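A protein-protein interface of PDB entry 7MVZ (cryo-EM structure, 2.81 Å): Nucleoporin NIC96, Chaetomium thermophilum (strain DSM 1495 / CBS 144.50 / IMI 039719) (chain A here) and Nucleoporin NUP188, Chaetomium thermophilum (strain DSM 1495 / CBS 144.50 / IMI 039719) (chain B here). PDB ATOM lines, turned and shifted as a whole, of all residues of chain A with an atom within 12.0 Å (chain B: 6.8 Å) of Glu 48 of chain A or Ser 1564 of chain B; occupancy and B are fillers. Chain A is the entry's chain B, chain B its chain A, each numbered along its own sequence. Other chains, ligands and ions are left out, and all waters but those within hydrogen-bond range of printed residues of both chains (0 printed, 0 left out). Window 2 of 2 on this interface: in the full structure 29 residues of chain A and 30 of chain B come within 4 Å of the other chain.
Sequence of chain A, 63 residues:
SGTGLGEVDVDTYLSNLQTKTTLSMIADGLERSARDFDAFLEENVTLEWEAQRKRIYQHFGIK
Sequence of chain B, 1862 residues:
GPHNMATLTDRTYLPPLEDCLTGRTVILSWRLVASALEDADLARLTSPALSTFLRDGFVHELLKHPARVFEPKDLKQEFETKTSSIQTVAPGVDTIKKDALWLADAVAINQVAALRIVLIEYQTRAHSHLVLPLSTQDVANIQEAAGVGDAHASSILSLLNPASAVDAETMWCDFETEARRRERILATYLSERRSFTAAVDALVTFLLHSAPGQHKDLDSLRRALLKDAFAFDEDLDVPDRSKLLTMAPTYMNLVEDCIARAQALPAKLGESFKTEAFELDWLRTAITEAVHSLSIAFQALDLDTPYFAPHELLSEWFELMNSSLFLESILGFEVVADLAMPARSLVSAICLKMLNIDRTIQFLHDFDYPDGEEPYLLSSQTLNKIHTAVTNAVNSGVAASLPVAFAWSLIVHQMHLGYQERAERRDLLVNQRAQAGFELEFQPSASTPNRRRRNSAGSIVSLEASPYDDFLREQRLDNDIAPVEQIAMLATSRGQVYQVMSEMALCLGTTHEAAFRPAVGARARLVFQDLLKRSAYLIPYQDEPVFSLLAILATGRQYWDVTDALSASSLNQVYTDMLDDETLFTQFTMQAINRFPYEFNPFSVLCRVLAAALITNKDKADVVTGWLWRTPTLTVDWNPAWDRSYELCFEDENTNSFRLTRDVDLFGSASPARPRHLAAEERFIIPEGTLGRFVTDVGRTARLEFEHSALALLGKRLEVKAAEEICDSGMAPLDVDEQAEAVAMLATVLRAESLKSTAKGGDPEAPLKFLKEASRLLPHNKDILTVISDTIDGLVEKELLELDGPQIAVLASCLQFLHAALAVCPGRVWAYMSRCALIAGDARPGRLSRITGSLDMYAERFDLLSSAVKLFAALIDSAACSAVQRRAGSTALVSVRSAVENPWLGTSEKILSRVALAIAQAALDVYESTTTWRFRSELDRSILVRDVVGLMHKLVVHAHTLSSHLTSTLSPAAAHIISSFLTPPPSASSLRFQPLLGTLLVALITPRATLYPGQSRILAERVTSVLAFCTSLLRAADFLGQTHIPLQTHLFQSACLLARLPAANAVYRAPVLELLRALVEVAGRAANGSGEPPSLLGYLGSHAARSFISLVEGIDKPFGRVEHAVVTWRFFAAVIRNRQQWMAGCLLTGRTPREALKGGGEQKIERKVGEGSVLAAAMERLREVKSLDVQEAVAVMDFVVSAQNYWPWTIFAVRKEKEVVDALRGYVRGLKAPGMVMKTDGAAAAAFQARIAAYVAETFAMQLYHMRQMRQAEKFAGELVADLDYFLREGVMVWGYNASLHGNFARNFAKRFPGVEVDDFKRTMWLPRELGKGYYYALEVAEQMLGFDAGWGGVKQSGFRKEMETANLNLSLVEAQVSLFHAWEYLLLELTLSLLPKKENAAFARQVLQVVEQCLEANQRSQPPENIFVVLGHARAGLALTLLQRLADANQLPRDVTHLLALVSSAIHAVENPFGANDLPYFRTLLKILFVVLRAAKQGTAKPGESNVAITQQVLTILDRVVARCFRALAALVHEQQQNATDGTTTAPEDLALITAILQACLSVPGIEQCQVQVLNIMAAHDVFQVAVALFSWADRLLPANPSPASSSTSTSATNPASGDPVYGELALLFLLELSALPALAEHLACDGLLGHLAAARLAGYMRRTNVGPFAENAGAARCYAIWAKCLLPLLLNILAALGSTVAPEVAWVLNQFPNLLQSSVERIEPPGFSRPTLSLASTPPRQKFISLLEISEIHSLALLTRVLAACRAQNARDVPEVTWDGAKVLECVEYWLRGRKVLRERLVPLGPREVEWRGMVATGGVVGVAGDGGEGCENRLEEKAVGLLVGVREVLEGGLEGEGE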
ATOM      1  N   ALA A  39     -11.746  -3.703  16.841  1.00  0.00           N
ATOM      2  CA  ALA A  39     -12.224  -4.536  15.740  1.00  0.00           C
ATOM      3  C   ALA A  39     -11.186  -4.669  14.634  1.00  0.00           C
ATOM      4  O   ALA A  39     -11.081  -5.727  14.002  1.00  0.00           O
ATOM      5  CB  ALA A  39     -13.523  -3.961  15.177  1.00  0.00           C
ATOM      6  N   PHE A  40     -10.383  -3.628  14.411  1.00  0.00           N
ATOM      7  CA  PHE A  40      -9.374  -3.697  13.358  1.00  0.00           C
ATOM      8  C   PHE A  40      -8.272  -4.680  13.731  1.00  0.00           C
ATOM      9  O   PHE A  40      -7.802  -5.448  12.885  1.00  0.00           O
ATOM     10  CB  PHE A  40      -8.812  -2.299  13.092  1.00  0.00           C
ATOM     11  CG  PHE A  40      -7.689  -2.269  12.095  1.00  0.00           C
ATOM     12  CD1 PHE A  40      -7.953  -2.303  10.736  1.00  0.00           C
ATOM     13  CD2 PHE A  40      -6.374  -2.152  12.514  1.00  0.00           C
ATOM     14  CE1 PHE A  40      -6.925  -2.258   9.814  1.00  0.00           C
ATOM     15  CE2 PHE A  40      -5.342  -2.104  11.593  1.00  0.00           C
ATOM     16  CZ  PHE A  40      -5.618  -2.157  10.244  1.00  0.00           C
ATOM     17  N   LEU A  41      -7.839  -4.655  14.989  1.00  0.00           N
ATOM     18  CA  LEU A  41      -6.889  -5.645  15.482  1.00  0.00           C
ATOM     19  C   LEU A  41      -7.464  -7.053  15.378  1.00  0.00           C
ATOM     20  O   LEU A  41      -6.754  -7.997  15.009  1.00  0.00           O
ATOM     21  CB  LEU A  41      -6.511  -5.312  16.927  1.00  0.00           C
ATOM     22  CG  LEU A  41      -5.271  -5.953  17.558  1.00  0.00           C
ATOM     23  CD1 LEU A  41      -4.902  -5.211  18.831  1.00  0.00           C
ATOM     24  CD2 LEU A  41      -5.484  -7.429  17.866  1.00  0.00           C
ATOM     25  N   GLU A  42      -8.737  -7.224  15.749  1.00  0.00           N
ATOM     26  CA  GLU A  42      -9.366  -8.535  15.621  1.00  0.00           C
ATOM     27  C   GLU A  42      -9.388  -9.008  14.172  1.00  0.00           C
ATOM     28  O   GLU A  42      -9.162 -10.195  13.898  1.00  0.00           O
ATOM     29  CB  GLU A  42     -10.787  -8.489  16.183  1.00  0.00           C
ATOM     30  CG  GLU A  42     -10.850  -8.275  17.687  1.00  0.00           C
ATOM     31  CD  GLU A  42     -12.272  -8.163  18.202  1.00  0.00           C
ATOM     32  OE1 GLU A  42     -13.200  -8.065  17.372  1.00  0.00           O
ATOM     33  OE2 GLU A  42     -12.461  -8.173  19.436  1.00  0.00           O
ATOM     34  N   GLU A  43      -9.550  -8.083  13.224  1.00  0.00           N
ATOM     35  CA  GLU A  43      -9.516  -8.478  11.821  1.00  0.00           C
ATOM     36  C   GLU A  43      -8.094  -8.801  11.389  1.00  0.00           C
ATOM     37  O   GLU A  43      -7.876  -9.720  10.592  1.00  0.00           O
ATOM     38  CB  GLU A  43     -10.109  -7.376  10.942  1.00  0.00           C
ATOM     39  CG  GLU A  43     -11.588  -7.119  11.182  1.00  0.00           C
ATOM     40  CD  GLU A  43     -12.460  -8.286  10.760  1.00  0.00           C
ATOM     41  OE1 GLU A  43     -11.931  -9.231  10.136  1.00  0.00           O
ATOM     42  OE2 GLU A  43     -13.673  -8.260  11.051  1.00  0.00           O
ATOM     43  N   ASN A  44      -7.115  -8.059  11.905  1.00  0.00           N
ATOM     44  CA  ASN A  44      -5.722  -8.387  11.633  1.00  0.00           C
ATOM     45  C   ASN A  44      -5.431  -9.818  12.063  1.00  0.00           C
ATOM     46  O   ASN A  44      -4.939 -10.635  11.277  1.00  0.00           O
ATOM     47  CB  ASN A  44      -4.795  -7.422  12.371  1.00  0.00           C
ATOM     48  CG  ASN A  44      -4.959  -5.991  11.920  1.00  0.00           C
ATOM     49  OD1 ASN A  44      -5.299  -5.719  10.769  1.00  0.00           O
ATOM     50  ND2 ASN A  44      -4.694  -5.061  12.828  1.00  0.00           N
ATOM     51  N   VAL A  45      -5.694 -10.123  13.336  1.00  0.00           N
ATOM     52  CA  VAL A  45      -5.355 -11.435  13.872  1.00  0.00           C
ATOM     53  C   VAL A  45      -6.191 -12.540  13.236  1.00  0.00           C
ATOM     54  O   VAL A  45      -5.715 -13.678  13.129  1.00  0.00           O
ATOM     55  CB  VAL A  45      -5.500 -11.456  15.407  1.00  0.00           C
ATOM     56  CG1 VAL A  45      -4.507 -10.495  16.045  1.00  0.00           C
ATOM     57  CG2 VAL A  45      -6.915 -11.119  15.831  1.00  0.00           C
ATOM     58  N   THR A  46      -7.361 -12.214  12.673  1.00  0.00           N
ATOM     59  CA  THR A  46      -8.114 -13.262  11.992  1.00  0.00           C
ATOM     60  C   THR A  46      -7.581 -13.495  10.586  1.00  0.00           C
ATOM     61  O   THR A  46      -7.458 -14.648  10.155  1.00  0.00           O
ATOM     62  CB  THR A  46      -9.599 -12.899  11.945  1.00  0.00           C
ATOM     63  OG1 THR A  46     -10.110 -12.792  13.279  1.00  0.00           O
ATOM     64  CG2 THR A  46     -10.387 -13.961  11.190  1.00  0.00           C
ATOM     65  N   LEU A  47      -7.193 -12.432   9.876  1.00  0.00           N
ATOM     66  CA  LEU A  47      -6.625 -12.638   8.553  1.00  0.00           C
ATOM     67  C   LEU A  47      -5.244 -13.258   8.678  1.00  0.00           C
ATOM     68  O   LEU A  47      -4.796 -13.956   7.764  1.00  0.00           O
ATOM     69  CB  LEU A  47      -6.577 -11.323   7.768  1.00  0.00           C
ATOM     70  CG  LEU A  47      -5.742 -10.151   8.296  1.00  0.00           C
ATOM     71  CD1 LEU A  47      -4.250 -10.347   8.047  1.00  0.00           C
ATOM     72  CD2 LEU A  47      -6.217  -8.846   7.674  1.00  0.00           C
ATOM     73  N   GLU A  48      -4.624 -13.119   9.852  1.00  0.00           N
ATOM     74  CA  GLU A  48      -3.322 -13.716  10.108  1.00  0.00           C
ATOM     75  C   GLU A  48      -3.471 -15.205  10.380  1.00  0.00           C
ATOM     76  O   GLU A  48      -2.742 -16.017   9.804  1.00  0.00           O
ATOM     77  CB  GLU A  48      -2.637 -13.013  11.282  1.00  0.00           C
ATOM     78  CG  GLU A  48      -1.313 -13.641  11.688  1.00  0.00           C
ATOM     79  CD  GLU A  48      -0.333 -13.729  10.536  1.00  0.00           C
ATOM     80  OE1 GLU A  48      -0.462 -12.936   9.579  1.00  0.00           O
ATOM     81  OE2 GLU A  48       0.569 -14.591  10.587  1.00  0.00           O
ATOM     82  N   TRP A  49      -4.330 -15.575  11.332  1.00  0.00           N
ATOM     83  CA  TRP A  49      -4.633 -16.988  11.522  1.00  0.00           C
ATOM     84  C   TRP A  49      -4.983 -17.639  10.186  1.00  0.00           C
ATOM     85  O   TRP A  49      -4.505 -18.735   9.867  1.00  0.00           O
ATOM     86  CB  TRP A  49      -5.780 -17.151  12.521  1.00  0.00           C
ATOM     87  CG  TRP A  49      -5.425 -16.744  13.923  1.00  0.00           C
ATOM     88  CD1 TRP A  49      -4.191 -16.393  14.388  1.00  0.00           C
ATOM     89  CD2 TRP A  49      -6.317 -16.648  15.040  1.00  0.00           C
ATOM     90  NE1 TRP A  49      -4.259 -16.085  15.725  1.00  0.00           N
ATOM     91  CE2 TRP A  49      -5.553 -16.234  16.150  1.00  0.00           C
ATOM     92  CE3 TRP A  49      -7.686 -16.874  15.212  1.00  0.00           C
ATOM     93  CZ2 TRP A  49      -6.112 -16.039  17.411  1.00  0.00           C
ATOM     94  CZ3 TRP A  49      -8.240 -16.680  16.465  1.00  0.00           C
ATOM     95  CH2 TRP A  49      -7.454 -16.267  17.547  1.00  0.00           C
ATOM     96  N   GLU A  50      -5.865 -16.993   9.413  1.00  0.00           N
ATOM     97  CA  GLU A  50      -6.212 -17.480   8.080  1.00  0.00           C
ATOM     98  C   GLU A  50      -4.974 -17.713   7.218  1.00  0.00           C
ATOM     99  O   GLU A  50      -4.802 -18.791   6.640  1.00  0.00           O
ATOM    100  CB  GLU A  50      -7.158 -16.486   7.401  1.00  0.00           C
ATOM    101  CG  GLU A  50      -7.660 -16.926   6.033  1.00  0.00           C
ATOM    102  CD  GLU A  50      -8.514 -18.178   6.095  1.00  0.00           C
ATOM    103  OE1 GLU A  50      -8.901 -18.583   7.212  1.00  0.00           O
ATOM    104  OE2 GLU A  50      -8.799 -18.759   5.027  1.00  0.00           O
ATOM    105  N   ALA A  51      -4.128 -16.689   7.077  1.00  0.00           N
ATOM    106  CA  ALA A  51      -2.903 -16.812   6.290  1.00  0.00           C
ATOM    107  C   ALA A  51      -2.050 -17.991   6.747  1.00  0.00           C
ATOM    108  O   ALA A  51      -1.543 -18.762   5.924  1.00  0.00           O
ATOM    109  CB  ALA A  51      -2.103 -15.511   6.373  1.00  0.00           C
ATOM    110  N   GLN A  52      -1.802 -18.083   8.053  1.00  0.00           N
ATOM    111  CA  GLN A  52      -1.036 -19.196   8.606  1.00  0.00           C
ATOM    112  C   GLN A  52      -1.623 -20.540   8.186  1.00  0.00           C
ATOM    113  O   GLN A  52      -0.913 -21.414   7.675  1.00  0.00           O
ATOM    114  CB  GLN A  52      -0.991 -19.080  10.132  1.00  0.00           C
ATOM    115  CG  GLN A  52      -0.159 -20.156  10.819  1.00  0.00           C
ATOM    116  CD  GLN A  52       1.304 -20.128  10.412  1.00  0.00           C
ATOM    117  OE1 GLN A  52       1.919 -21.173  10.202  1.00  0.00           O
ATOM    118  NE2 GLN A  52       1.870 -18.930  10.307  1.00  0.00           N
ATOM    119  N   ARG A  53      -2.912 -20.745   8.460  1.00  0.00           N
ATOM    120  CA  ARG A  53      -3.566 -21.982   8.042  1.00  0.00           C
ATOM    121  C   ARG A  53      -3.380 -22.229   6.549  1.00  0.00           C
ATOM    122  O   ARG A  53      -3.163 -23.366   6.121  1.00  0.00           O
ATOM    123  CB  ARG A  53      -5.048 -21.941   8.413  1.00  0.00           C
ATOM    124  CG  ARG A  53      -5.865 -23.089   7.847  1.00  0.00           C
ATOM    125  CD  ARG A  53      -7.305 -23.012   8.309  1.00  0.00           C
ATOM    126  NE  ARG A  53      -8.176 -23.905   7.553  1.00  0.00           N
ATOM    127  CZ  ARG A  53      -9.489 -23.996   7.735  1.00  0.00           C
ATOM    128  NH1 ARG A  53     -10.203 -24.835   6.996  1.00  0.00           N
ATOM    129  NH2 ARG A  53     -10.085 -23.256   8.661  1.00  0.00           N
ATOM    130  N   LYS A  54      -3.487 -21.174   5.739  1.00  0.00           N
ATOM    131  CA  LYS A  54      -3.280 -21.305   4.299  1.00  0.00           C
ATOM    132  C   LYS A  54      -1.883 -21.832   3.988  1.00  0.00           C
ATOM    133  O   LYS A  54      -1.717 -22.757   3.185  1.00  0.00           O
ATOM    134  CB  LYS A  54      -3.512 -19.956   3.615  1.00  0.00           C
ATOM    135  CG  LYS A  54      -3.473 -20.007   2.092  1.00  0.00           C
ATOM    136  CD  LYS A  54      -4.595 -20.862   1.524  1.00  0.00           C
ATOM    137  CE  LYS A  54      -4.599 -20.834   0.003  1.00  0.00           C
ATOM    138  NZ  LYS A  54      -5.685 -21.677  -0.570  1.00  0.00           N
ATOM    139  N   ARG A  55      -0.859 -21.214   4.578  1.00  0.00           N
ATOM    140  CA  ARG A  55       0.507 -21.643   4.297  1.00  0.00           C
ATOM    141  C   ARG A  55       0.732 -23.078   4.756  1.00  0.00           C
ATOM    142  O   ARG A  55       1.484 -23.821   4.120  1.00  0.00           O
ATOM    143  CB  ARG A  55       1.517 -20.697   4.953  1.00  0.00           C
ATOM    144  CG  ARG A  55       1.963 -21.085   6.357  1.00  0.00           C
ATOM    145  CD  ARG A  55       2.866 -20.024   6.966  1.00  0.00           C
ATOM    146  NE  ARG A  55       2.196 -18.732   7.091  1.00  0.00           N
ATOM    147  CZ  ARG A  55       2.773 -17.630   7.560  1.00  0.00           C
ATOM    148  NH1 ARG A  55       4.040 -17.654   7.954  1.00  0.00           N
ATOM    149  NH2 ARG A  55       2.083 -16.500   7.637  1.00  0.00           N
ATOM    150  N   ILE A  56       0.092 -23.490   5.850  1.00  0.00           N
ATOM    151  CA  ILE A  56       0.170 -24.892   6.257  1.00  0.00           C
ATOM    152  C   ILE A  56      -0.505 -25.790   5.221  1.00  0.00           C
ATOM    153  O   ILE A  56      -0.004 -26.873   4.887  1.00  0.00           O
ATOM    154  CB  ILE A  56      -0.445 -25.072   7.658  1.00  0.00           C
ATOM    155  CG1 ILE A  56       0.306 -24.207   8.677  1.00  0.00           C
ATOM    156  CG2 ILE A  56      -0.421 -26.540   8.065  1.00  0.00           C
ATOM    157  CD1 ILE A  56      -0.268 -24.247  10.082  1.00  0.00           C
ATOM    158  N   TYR A  57      -1.659 -25.355   4.705  1.00  0.00           N
ATOM    159  CA  TYR A  57      -2.350 -26.092   3.650  1.00  0.00           C
ATOM    160  C   TYR A  57      -1.509 -26.203   2.387  1.00  0.00           C
ATOM    161  O   TYR A  57      -1.669 -27.157   1.617  1.00  0.00           O
ATOM    162  CB  TYR A  57      -3.679 -25.407   3.334  1.00  0.00           C
ATOM    163  CG  TYR A  57      -4.483 -26.090   2.253  1.00  0.00           C
ATOM    164  CD1 TYR A  57      -5.343 -27.139   2.547  1.00  0.00           C
ATOM    165  CD2 TYR A  57      -4.392 -25.666   0.934  1.00  0.00           C
ATOM    166  CE1 TYR A  57      -6.081 -27.754   1.551  1.00  0.00           C
ATOM    167  CE2 TYR A  57      -5.123 -26.273  -0.064  1.00  0.00           C
ATOM    168  CZ  TYR A  57      -5.964 -27.315   0.248  1.00  0.00           C
ATOM    169  OH  TYR A  57      -6.690 -27.914  -0.754  1.00  0.00           O
ATOM    170  N   LYS B1498       4.499  -5.745   7.000  1.00  0.00           N
ATOM    171  CA  LYS B1498       4.109  -7.070   6.529  1.00  0.00           C
ATOM    172  C   LYS B1498       3.507  -7.010   5.132  1.00  0.00           C
ATOM    173  O   LYS B1498       3.697  -7.936   4.335  1.00  0.00           O
ATOM    174  CB  LYS B1498       3.120  -7.703   7.511  1.00  0.00           C
ATOM    175  CG  LYS B1498       2.625  -9.086   7.105  1.00  0.00           C
ATOM    176  CD  LYS B1498       1.290  -9.019   6.372  1.00  0.00           C
ATOM    177  CE  LYS B1498       0.769 -10.408   6.039  1.00  0.00           C
ATOM    178  NZ  LYS B1498       1.701 -11.158   5.153  1.00  0.00           N
ATOM    179  N   LEU B1559       3.266  -9.696  18.752  1.00  0.00           N
ATOM    180  CA  LEU B1559       4.093 -10.819  18.321  1.00  0.00           C
ATOM    181  C   LEU B1559       3.451 -11.563  17.156  1.00  0.00           C
ATOM    182  O   LEU B1559       4.138 -11.958  16.205  1.00  0.00           O
ATOM    183  CB  LEU B1559       4.342 -11.767  19.495  1.00  0.00           C
ATOM    184  CG  LEU B1559       5.166 -13.021  19.191  1.00  0.00           C
ATOM    185  CD1 LEU B1559       6.511 -12.664  18.578  1.00  0.00           C
ATOM    186  CD2 LEU B1559       5.363 -13.845  20.451  1.00  0.00           C
ATOM    187  N   GLN B1560       2.130 -11.755  17.206  1.00  0.00           N
ATOM    188  CA  GLN B1560       1.439 -12.446  16.123  1.00  0.00           C
ATOM    189  C   GLN B1560       1.605 -11.701  14.804  1.00  0.00           C
ATOM    190  O   GLN B1560       1.951 -12.297  13.778  1.00  0.00           O
ATOM    191  CB  GLN B1560      -0.042 -12.610  16.471  1.00  0.00           C
ATOM    192  CG  GLN B1560      -0.845 -13.389  15.440  1.00  0.00           C
ATOM    193  CD  GLN B1560      -2.334 -13.410  15.740  1.00  0.00           C
ATOM    194  OE1 GLN B1560      -3.161 -13.366  14.829  1.00  0.00           O
ATOM    195  NE2 GLN B1560      -2.684 -13.488  17.020  1.00  0.00           N
ATOM    196  N   ALA B1561       1.361 -10.389  14.813  1.00  0.00           N
ATOM    197  CA  ALA B1561       1.477  -9.601  13.592  1.00  0.00           C
ATOM    198  C   ALA B1561       2.923  -9.421  13.151  1.00  0.00           C
ATOM    199  O   ALA B1561       3.168  -9.162  11.967  1.00  0.00           O
ATOM    200  CB  ALA B1561       0.819  -8.235  13.786  1.00  0.00           C
ATOM    201  N   CYS B1562       3.885  -9.551  14.068  1.00  0.00           N
ATOM    202  CA  CYS B1562       5.287  -9.402  13.700  1.00  0.00           C
ATOM    203  C   CYS B1562       5.858 -10.682  13.110  1.00  0.00           C
ATOM    204  O   CYS B1562       6.728 -10.620  12.235  1.00  0.00           O
ATOM    205  CB  CYS B1562       6.104  -8.982  14.925  1.00  0.00           C
ATOM    206  SG  CYS B1562       7.869  -8.733  14.609  1.00  0.00           S
ATOM    207  N   LEU B1563       5.381 -11.842  13.561  1.00  0.00           N
ATOM    208  CA  LEU B1563       5.842 -13.111  13.008  1.00  0.00           C
ATOM    209  C   LEU B1563       5.315 -13.373  11.601  1.00  0.00           C
ATOM    210  O   LEU B1563       5.619 -14.432  11.038  1.00  0.00           O
ATOM    211  CB  LEU B1563       5.430 -14.260  13.932  1.00  0.00           C
ATOM    212  CG  LEU B1563       6.142 -14.340  15.285  1.00  0.00           C
ATOM    213  CD1 LEU B1563       5.505 -15.412  16.154  1.00  0.00           C
ATOM    214  CD2 LEU B1563       7.631 -14.608  15.113  1.00  0.00           C
ATOM    215  N   SER B1564       4.545 -12.452  11.025  1.00  0.00           N
ATOM    216  CA  SER B1564       3.945 -12.636   9.710  1.00  0.00           C
ATOM    217  C   SER B1564       4.718 -11.945   8.595  1.00  0.00           C
ATOM    218  O   SER B1564       4.320 -12.048   7.432  1.00  0.00           O
ATOM    219  CB  SER B1564       2.503 -12.122   9.721  1.00  0.00           C
ATOM    220  OG  SER B1564       1.865 -12.364   8.480  1.00  0.00           O
ATOM    221  N   VAL B1565       5.802 -11.249   8.913  1.00  0.00           N
ATOM    222  CA  VAL B1565       6.562 -10.547   7.871  1.00  0.00           C
ATOM    223  C   VAL B1565       7.222 -11.574   6.958  1.00  0.00           C
ATOM    224  O   VAL B1565       7.731 -12.596   7.452  1.00  0.00           O
ATOM    225  CB  VAL B1565       7.603  -9.620   8.504  1.00  0.00           C
ATOM    226  CG1 VAL B1565       8.341  -8.829   7.431  1.00  0.00           C
ATOM    227  CG2 VAL B1565       6.943  -8.672   9.500  1.00  0.00           C
ATOM    228  N   PRO B1566       7.240 -11.364   5.637  1.00  0.00           N
ATOM    229  CA  PRO B1566       7.827 -12.385   4.752  1.00  0.00           C
ATOM    230  C   PRO B1566       9.288 -12.675   5.048  1.00  0.00           C
ATOM    231  O   PRO B1566       9.744 -13.804   4.826  1.00  0.00           O
ATOM    232  CB  PRO B1566       7.646 -11.782   3.351  1.00  0.00           C
ATOM    233  CG  PRO B1566       6.551 -10.787   3.493  1.00  0.00           C
ATOM    234  CD  PRO B1566       6.681 -10.234   4.875  1.00  0.00           C
ATOM    235  N   GLY B1567      10.038 -11.690   5.542  1.00  0.00           N
ATOM    236  CA  GLY B1567      11.446 -11.886   5.843  1.00  0.00           C
ATOM    237  C   GLY B1567      11.722 -12.875   6.956  1.00  0.00           C
ATOM    238  O   GLY B1567      12.886 -13.230   7.167  1.00  0.00           O
ATOM    239  N   ILE B1568      10.688 -13.326   7.667  1.00  0.00           N
ATOM    240  CA  ILE B1568      10.880 -14.256   8.774  1.00  0.00           C
ATOM    241  C   ILE B1568      10.748 -15.713   8.343  1.00  0.00           C
ATOM    242  O   ILE B1568      11.278 -16.600   9.026  1.00  0.00           O
ATOM    243  CB  ILE B1568       9.889 -13.943   9.911  1.00  0.00           C
ATOM    244  CG1 ILE B1568      10.096 -12.506  10.401  1.00  0.00           C
ATOM    245  CG2 ILE B1568      10.053 -14.930  11.068  1.00  0.00           C
ATOM    246  CD1 ILE B1568       9.078 -12.042  11.418  1.00  0.00           C
ATOM    247  N   GLU B1569      10.072 -15.987   7.225  1.00  0.00           N
ATOM    248  CA  GLU B1569       9.890 -17.363   6.780  1.00  0.00           C
ATOM    249  C   GLU B1569      11.195 -18.021   6.350  1.00  0.00           C
ATOM    250  O   GLU B1569      11.212 -19.238   6.135  1.00  0.00           O
ATOM    251  CB  GLU B1569       8.889 -17.410   5.624  1.00  0.00           C
ATOM    252  CG  GLU B1569       7.511 -16.874   5.979  1.00  0.00           C
ATOM    253  CD  GLU B1569       6.544 -16.933   4.814  1.00  0.00           C
ATOM    254  OE1 GLU B1569       6.948 -17.397   3.726  1.00  0.00           O
ATOM    255  OE2 GLU B1569       5.379 -16.516   4.985  1.00  0.00           O
ATOM    256  N   ALA B1637       4.037 -20.902  15.704  1.00  0.00           N
ATOM    257  CA  ALA B1637       3.889 -20.655  14.275  1.00  0.00           C
ATOM    258  C   ALA B1637       5.125 -21.064  13.482  1.00  0.00           C
ATOM    259  O   ALA B1637       5.025 -21.270  12.267  1.00  0.00           O
ATOM    260  CB  ALA B1637       3.583 -19.178  14.028  1.00  0.00           C
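OE1 of Gln 1560 of chain B lies close to O of Val 45 of chain A (3.1 Å).
The indole nitrogen of Trp 49 of chain A sits at hydrogen-bond distance from the side-chain amide oxygen of Gln 1560 of chain B (3.1 Å).
OG of Ser 1564 of chain B is in hydrogen-bond range of OE1 of Glu 48 of chain A (2.6 Å).
OE2 of Glu 1569 of chain B is in salt-bridge range of NH1 of Arg 55 of chain A.
OE2 of Glu 48 of chain A is in salt-bridge range of NH2 of Arg 55 of chain A, at 3.8 Å.
The side-chain amide nitrogen (NE2) of Gln 52 of chain A lies close to the guanidinium group (NE) of Arg 55 of chain A (3.2 Å).
Among the printed residues, merely in contact across the chains: Glu 48 of chain A with Gln 1560 of chain B and Gln 52 of chain A with Ala 1637 of chain B.
Glu 48 of chain A touches just these residues of chain B: Gln 1560 and Ser 1564.
No residue of chain A comes within 4 Å of Leu 1563 of chain B.
No residue of chain A comes within 4 Å of Pro 1566 of chain B.
Printed residues of chain A within 4 Å of Ala 1637 of chain B: Gln 52 (3.7 Å).
Printed residues of chain A within 4 Å of Glu 1569 of chain B: Arg 55.
Glu 42 of chain A touches none of the printed residues of chain B.
Leu 1559 of chain B touches none of the printed residues of chain A.
The nearest residue of chain B that does not touch Glu 48 of chain A is Lys 1498 of chain B (4.5 Å).
Of the 19 printed residues of chain A, 5 touch a printed residue of chain B.
Hydrophobic or aromatic side chains of chain A that line the printed part of chain B: Val 45 and Trp 49.
Of the 13 printed residues of chain B, 4 touch a printed residue of chain A.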
